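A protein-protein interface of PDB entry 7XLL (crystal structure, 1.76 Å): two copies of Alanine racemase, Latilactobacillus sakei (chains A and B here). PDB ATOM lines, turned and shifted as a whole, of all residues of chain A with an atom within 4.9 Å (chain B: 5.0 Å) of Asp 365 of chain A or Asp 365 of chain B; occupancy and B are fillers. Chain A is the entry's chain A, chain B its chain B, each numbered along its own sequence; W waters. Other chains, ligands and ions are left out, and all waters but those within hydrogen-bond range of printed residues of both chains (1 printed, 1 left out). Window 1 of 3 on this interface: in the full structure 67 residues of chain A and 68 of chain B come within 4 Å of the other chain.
OD1 of Asp 365 of chain A lies close to OD1 of Asp 365 of chain B (2.7 Å).
Water W1 lies within hydrogen-bond range of the side-chain carboxylate (OD1) of Asp 365 of chain B, the backbone carbonyl oxygen (O) of Tyr 290 of chain A and the backbone NH (N) of Gly 293 of chain A.
Tyr 290 of chain A touches Glu 361 of chain B, and with the chains exchanged Glu 361 of chain A touches Tyr 290 of chain B. Leu 295 of chain A touches its own counterpart, Leu 295 of chain B. Leu 295 of chain A touches Glu 361 of chain B, and with the chains exchanged Glu 361 of chain A touches Leu 295 of chain B. Asp 365 of chain A touches its own counterpart, Asp 365 of chain B. 11 positions are printed for both chains. Of the 8 pairs that touch across the chains among the printed residues, 8 have their exchanged pair printed and touching as well.
Of the 11 printed residues of chain B, 4 touch a printed residue of chain A. Hydrophobic or aromatic side chains of chain B that line the printed part of chain A: Tyr 290 and Leu 295. Of the 11 printed residues of chain A, 4 touch a printed residue of chain B.
Among the printed residues, merely in contact across the chains: Tyr 290 of chain A with Glu 361 of chain B, Leu 295 of chain A with Leu 295 of chain B, Leu 295 of chain A with Glu 361 of chain B, Leu 295 of chain A with Asp 365 of chain B, Glu 361 of chain A with Tyr 290 of chain B, Glu 361 of chain A with Leu 295 of chain B and Asp 365 of chain A with Leu 295 of chain B.
Of chain B, only Leu 295 (3.8 Å) and Asp 365 (2.7 Å) come within 4 Å of Asp 365 of chain A. Of chain A, only Leu 295 and Asp 365 come within 4 Å of Asp 365 of chain B. Of the printed residues of chain A, Tyr 290 of chain B touches Glu 361. Of the printed residues of chain B, Leu 295 of chain A touches Leu 295 (3.4 Å), Glu 361 (3.4 Å) and Asp 365 (3.95 Å). The nearest residue of chain B that does not touch Asp 365 of chain A is Gly 293 of chain B (4.6 Å). The nearest printed residue of chain A that does not touch Leu 295 of chain B is Cys 364 of chain A (6.8 Å).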
ATOM      1  N   TYR A 290       2.143 -17.734  -0.457  1.00  0.00           N
ATOM      2  CA  TYR A 290       1.648 -18.359   0.767  1.00  0.00           C
ATOM      3  C   TYR A 290       2.697 -18.383   1.879  1.00  0.00           C
ATOM      4  O   TYR A 290       2.324 -18.450   3.055  1.00  0.00           O
ATOM      5  CB  TYR A 290       1.079 -19.766   0.478  1.00  0.00           C
ATOM      6  CG  TYR A 290       2.006 -20.811  -0.125  1.00  0.00           C
ATOM      7  CD1 TYR A 290       3.001 -21.421   0.636  1.00  0.00           C
ATOM      8  CD2 TYR A 290       1.840 -21.232  -1.445  1.00  0.00           C
ATOM      9  CE1 TYR A 290       3.839 -22.395   0.082  1.00  0.00           C
ATOM     10  CE2 TYR A 290       2.654 -22.212  -2.000  1.00  0.00           C
ATOM     11  CZ  TYR A 290       3.659 -22.786  -1.236  1.00  0.00           C
ATOM     12  OH  TYR A 290       4.485 -23.755  -1.792  1.00  0.00           O
ATOM     13  N   ASP A 292       4.216 -15.852   2.823  1.00  0.00           N
ATOM     14  CA  ASP A 292       3.947 -14.591   3.492  1.00  0.00           C
ATOM     15  C   ASP A 292       2.660 -14.616   4.307  1.00  0.00           C
ATOM     16  O   ASP A 292       2.380 -13.661   5.042  1.00  0.00           O
ATOM     17  CB  ASP A 292       3.891 -13.475   2.450  1.00  0.00           C
ATOM     18  CG  ASP A 292       5.209 -13.311   1.716  1.00  0.00           C
ATOM     19  OD1 ASP A 292       6.237 -13.104   2.388  1.00  0.00           O
ATOM     20  OD2 ASP A 292       5.211 -13.397   0.471  1.00  0.00           O
ATOM     21  N   GLY A 293       1.877 -15.681   4.202  1.00  0.00           N
ATOM     22  CA  GLY A 293       0.574 -15.723   4.835  1.00  0.00           C
ATOM     23  C   GLY A 293      -0.592 -15.486   3.896  1.00  0.00           C
ATOM     24  O   GLY A 293      -1.742 -15.463   4.356  1.00  0.00           O
ATOM     25  N   LEU A 295      -2.429 -17.416   1.805  1.00  0.00           N
ATOM     26  CA  LEU A 295      -2.430 -18.853   1.588  1.00  0.00           C
ATOM     27  C   LEU A 295      -3.133 -19.222   0.287  1.00  0.00           C
ATOM     28  O   LEU A 295      -3.876 -18.433  -0.307  1.00  0.00           O
ATOM     29  CB  LEU A 295      -3.096 -19.560   2.772  1.00  0.00           C
ATOM     30  CG  LEU A 295      -2.456 -19.232   4.117  1.00  0.00           C
ATOM     31  CD1 LEU A 295      -3.051 -20.129   5.176  1.00  0.00           C
ATOM     32  CD2 LEU A 295      -0.941 -19.440   4.069  1.00  0.00           C
ATOM     33  N   GLU A 361      -7.359 -14.579  12.419  1.00  0.00           N
ATOM     34  CA  GLU A 361      -6.377 -15.503  11.866  1.00  0.00           C
ATOM     35  C   GLU A 361      -5.674 -14.905  10.660  1.00  0.00           C
ATOM     36  O   GLU A 361      -4.473 -15.143  10.460  1.00  0.00           O
ATOM     37  CB  GLU A 361      -7.035 -16.818  11.480  1.00  0.00           C
ATOM     38  CG  GLU A 361      -6.066 -17.819  10.834  1.00  0.00           C
ATOM     39  CD  GLU A 361      -6.724 -19.174  10.661  1.00  0.00           C
ATOM     40  OE1 GLU A 361      -7.370 -19.403   9.613  1.00  0.00           O
ATOM     41  OE2 GLU A 361      -6.645 -19.986  11.603  1.00  0.00           O
ATOM     42  N   ILE A 362      -6.397 -14.138   9.841  1.00  0.00           N
ATOM     43  CA  ILE A 362      -5.758 -13.498   8.690  1.00  0.00           C
ATOM     44  C   ILE A 362      -4.569 -12.657   9.143  1.00  0.00           C
ATOM     45  O   ILE A 362      -3.466 -12.769   8.592  1.00  0.00           O
ATOM     46  CB  ILE A 362      -6.771 -12.654   7.888  1.00  0.00           C
ATOM     47  CG1 ILE A 362      -7.940 -13.513   7.404  1.00  0.00           C
ATOM     48  CG2 ILE A 362      -6.084 -11.981   6.682  1.00  0.00           C
ATOM     49  CD1 ILE A 362      -7.542 -14.593   6.441  1.00  0.00           C
ATOM     50  N   ILE A 363      -4.775 -11.792  10.145  1.00  0.00           N
ATOM     51  CA  ILE A 363      -3.699 -10.882  10.533  1.00  0.00           C
ATOM     52  C   ILE A 363      -2.619 -11.622  11.309  1.00  0.00           C
ATOM     53  O   ILE A 363      -1.434 -11.280  11.210  1.00  0.00           O
ATOM     54  CB  ILE A 363      -4.229  -9.681  11.343  1.00  0.00           C
ATOM     55  CG1 ILE A 363      -4.945 -10.141  12.615  1.00  0.00           C
ATOM     56  CG2 ILE A 363      -5.133  -8.826  10.492  1.00  0.00           C
ATOM     57  CD1 ILE A 363      -5.731  -9.023  13.345  1.00  0.00           C
ATOM     58  N   CYS A 364      -2.995 -12.633  12.103  1.00  0.00           N
ATOM     59  CA  CYS A 364      -1.988 -13.348  12.875  1.00  0.00           C
ATOM     60  C   CYS A 364      -1.121 -14.240  11.995  1.00  0.00           C
ATOM     61  O   CYS A 364      -0.019 -14.616  12.414  1.00  0.00           O
ATOM     62  CB  CYS A 364      -2.670 -14.165  13.985  1.00  0.00           C
ATOM     63  SG  CYS A 364      -3.187 -13.184  15.398  1.00  0.00           S
ATOM     64  N   ASP A 365      -1.570 -14.541  10.777  1.00  0.00           N
ATOM     65  CA  ASP A 365      -0.849 -15.416   9.863  1.00  0.00           C
ATOM     66  C   ASP A 365       0.136 -14.670   8.975  1.00  0.00           C
ATOM     67  O   ASP A 365       0.838 -15.306   8.180  1.00  0.00           O
ATOM     68  CB  ASP A 365      -1.842 -16.183   8.972  1.00  0.00           C
ATOM     69  CG  ASP A 365      -1.301 -17.522   8.506  1.00  0.00           C
ATOM     70  OD1 ASP A 365      -0.518 -18.128   9.254  1.00  0.00           O
ATOM     71  OD2 ASP A 365      -1.676 -17.970   7.402  1.00  0.00           O
ATOM     72  N   LEU A 366       0.206 -13.346   9.085  1.00  0.00           N
ATOM     73  CA  LEU A 366       1.079 -12.566   8.214  1.00  0.00           C
ATOM     74  C   LEU A 366       2.532 -12.750   8.629  1.00  0.00           C
ATOM     75  O   LEU A 366       2.908 -12.436   9.762  1.00  0.00           O
ATOM     76  CB  LEU A 366       0.685 -11.097   8.265  1.00  0.00           C
ATOM     77  CG  LEU A 366      -0.749 -10.866   7.816  1.00  0.00           C
ATOM     78  CD1 LEU A 366      -1.146  -9.420   8.106  1.00  0.00           C
ATOM     79  CD2 LEU A 366      -0.881 -11.207   6.332  1.00  0.00           C
ATOM     80  N   SER A 367       3.352 -13.221   7.694  1.00  0.00           N
ATOM     81  CA  SER A 367       4.726 -13.583   7.994  1.00  0.00           C
ATOM     82  C   SER A 367       5.566 -12.363   8.362  1.00  0.00           C
ATOM     83  O   SER A 367       5.352 -11.257   7.860  1.00  0.00           O
ATOM     84  CB  SER A 367       5.354 -14.265   6.778  1.00  0.00           C
ATOM     85  OG  SER A 367       6.756 -14.222   6.859  1.00  0.00           O
ATOM     86  N   TYR B 290      -3.489 -20.838  16.298  1.00  0.00           N
ATOM     87  CA  TYR B 290      -3.385 -20.460  14.893  1.00  0.00           C
ATOM     88  C   TYR B 290      -2.367 -19.347  14.664  1.00  0.00           C
ATOM     89  O   TYR B 290      -1.832 -19.239  13.553  1.00  0.00           O
ATOM     90  CB  TYR B 290      -4.756 -20.085  14.310  1.00  0.00           C
ATOM     91  CG  TYR B 290      -5.539 -18.970  14.983  1.00  0.00           C
ATOM     92  CD1 TYR B 290      -5.211 -17.628  14.784  1.00  0.00           C
ATOM     93  CD2 TYR B 290      -6.654 -19.261  15.767  1.00  0.00           C
ATOM     94  CE1 TYR B 290      -5.958 -16.609  15.388  1.00  0.00           C
ATOM     95  CE2 TYR B 290      -7.403 -18.263  16.360  1.00  0.00           C
ATOM     96  CZ  TYR B 290      -7.052 -16.938  16.178  1.00  0.00           C
ATOM     97  OH  TYR B 290      -7.807 -15.948  16.783  1.00  0.00           O
ATOM     98  N   ASP B 292       0.499 -19.493  15.717  1.00  0.00           N
ATOM     99  CA  ASP B 292       1.713 -20.249  15.440  1.00  0.00           C
ATOM    100  C   ASP B 292       1.687 -20.925  14.077  1.00  0.00           C
ATOM    101  O   ASP B 292       2.699 -21.506  13.657  1.00  0.00           O
ATOM    102  CB  ASP B 292       1.932 -21.300  16.532  1.00  0.00           C
ATOM    103  CG  ASP B 292       2.094 -20.680  17.895  1.00  0.00           C
ATOM    104  OD1 ASP B 292       3.052 -19.897  18.084  1.00  0.00           O
ATOM    105  OD2 ASP B 292       1.247 -20.962  18.767  1.00  0.00           O
ATOM    106  N   GLY B 293       0.569 -20.860  13.371  1.00  0.00           N
ATOM    107  CA  GLY B 293       0.447 -21.548  12.107  1.00  0.00           C
ATOM    108  C   GLY B 293      -0.321 -22.850  12.176  1.00  0.00           C
ATOM    109  O   GLY B 293      -0.410 -23.548  11.159  1.00  0.00           O
ATOM    110  N   LEU B 295      -3.603 -23.633  11.999  1.00  0.00           N
ATOM    111  CA  LEU B 295      -4.753 -22.804  11.714  1.00  0.00           C
ATOM    112  C   LEU B 295      -6.044 -23.494  12.145  1.00  0.00           C
ATOM    113  O   LEU B 295      -6.088 -24.700  12.404  1.00  0.00           O
ATOM    114  CB  LEU B 295      -4.809 -22.464  10.226  1.00  0.00           C
ATOM    115  CG  LEU B 295      -3.552 -21.797   9.675  1.00  0.00           C
ATOM    116  CD1 LEU B 295      -3.827 -21.382   8.249  1.00  0.00           C
ATOM    117  CD2 LEU B 295      -3.178 -20.596  10.527  1.00  0.00           C
ATOM    118  N   GLU B 361       2.960 -25.566   2.160  1.00  0.00           N
ATOM    119  CA  GLU B 361       2.317 -24.451   2.850  1.00  0.00           C
ATOM    120  C   GLU B 361       2.303 -24.662   4.357  1.00  0.00           C
ATOM    121  O   GLU B 361       2.486 -23.703   5.118  1.00  0.00           O
ATOM    122  CB  GLU B 361       0.903 -24.256   2.320  1.00  0.00           C
ATOM    123  CG  GLU B 361       0.114 -23.185   3.070  1.00  0.00           C
ATOM    124  CD  GLU B 361      -1.164 -22.855   2.362  1.00  0.00           C
ATOM    125  OE1 GLU B 361      -2.214 -23.457   2.718  1.00  0.00           O
ATOM    126  OE2 GLU B 361      -1.118 -22.034   1.419  1.00  0.00           O
ATOM    127  N   ILE B 362       2.069 -25.900   4.804  1.00  0.00           N
ATOM    128  CA  ILE B 362       2.113 -26.209   6.237  1.00  0.00           C
ATOM    129  C   ILE B 362       3.440 -25.753   6.842  1.00  0.00           C
ATOM    130  O   ILE B 362       3.471 -25.075   7.875  1.00  0.00           O
ATOM    131  CB  ILE B 362       1.872 -27.711   6.476  1.00  0.00           C
ATOM    132  CG1 ILE B 362       0.497 -28.152   5.938  1.00  0.00           C
ATOM    133  CG2 ILE B 362       1.970 -28.053   7.982  1.00  0.00           C
ATOM    134  CD1 ILE B 362      -0.661 -27.415   6.536  1.00  0.00           C
ATOM    135  N   ILE B 363       4.560 -26.097   6.198  1.00  0.00           N
ATOM    136  CA  ILE B 363       5.847 -25.774   6.814  1.00  0.00           C
ATOM    137  C   ILE B 363       6.191 -24.292   6.674  1.00  0.00           C
ATOM    138  O   ILE B 363       6.772 -23.702   7.592  1.00  0.00           O
ATOM    139  CB  ILE B 363       6.966 -26.669   6.250  1.00  0.00           C
ATOM    140  CG1 ILE B 363       7.072 -26.546   4.725  1.00  0.00           C
ATOM    141  CG2 ILE B 363       6.728 -28.102   6.683  1.00  0.00           C
ATOM    142  CD1 ILE B 363       8.218 -27.359   4.127  1.00  0.00           C
ATOM    143  N   CYS B 364       5.865 -23.660   5.537  1.00  0.00           N
ATOM    144  CA  CYS B 364       6.159 -22.234   5.402  1.00  0.00           C
ATOM    145  C   CYS B 364       5.275 -21.370   6.296  1.00  0.00           C
ATOM    146  O   CYS B 364       5.622 -20.211   6.557  1.00  0.00           O
ATOM    147  CB  CYS B 364       6.018 -21.779   3.948  1.00  0.00           C
ATOM    148  SG  CYS B 364       7.252 -22.473   2.832  1.00  0.00           S
ATOM    149  N   ASP B 365       4.156 -21.900   6.783  1.00  0.00           N
ATOM    150  CA  ASP B 365       3.234 -21.136   7.613  1.00  0.00           C
ATOM    151  C   ASP B 365       3.542 -21.273   9.095  1.00  0.00           C
ATOM    152  O   ASP B 365       2.811 -20.713   9.920  1.00  0.00           O
ATOM    153  CB  ASP B 365       1.788 -21.578   7.334  1.00  0.00           C
ATOM    154  CG  ASP B 365       0.761 -20.494   7.632  1.00  0.00           C
ATOM    155  OD1 ASP B 365       1.061 -19.295   7.471  1.00  0.00           O
ATOM    156  OD2 ASP B 365      -0.359 -20.855   8.041  1.00  0.00           O
ATOM    157  N   LEU B 366       4.601 -21.994   9.454  1.00  0.00           N
ATOM    158  CA  LEU B 366       4.964 -22.135  10.860  1.00  0.00           C
ATOM    159  C   LEU B 366       5.571 -20.831  11.356  1.00  0.00           C
ATOM    160  O   LEU B 366       6.547 -20.330  10.787  1.00  0.00           O
ATOM    161  CB  LEU B 366       5.936 -23.296  11.048  1.00  0.00           C
ATOM    162  CG  LEU B 366       5.317 -24.638  10.652  1.00  0.00           C
ATOM    163  CD1 LEU B 366       6.386 -25.718  10.581  1.00  0.00           C
ATOM    164  CD2 LEU B 366       4.179 -25.033  11.619  1.00  0.00           C
ATOM    165  N   SER B 367       4.991 -20.275  12.411  1.00  0.00           N
ATOM    166  CA  SER B 367       5.430 -18.976  12.902  1.00  0.00           C
ATOM    167  C   SER B 367       6.831 -19.047  13.511  1.00  0.00           C
ATOM    168  O   SER B 367       7.248 -20.066  14.072  1.00  0.00           O
ATOM    169  CB  SER B 367       4.433 -18.457  13.942  1.00  0.00           C
ATOM    170  OG  SER B 367       4.993 -17.424  14.721  1.00  0.00           O
HETATM  171  O   HOH W   1       2.516 -18.384   5.780  1.00  0.00           O
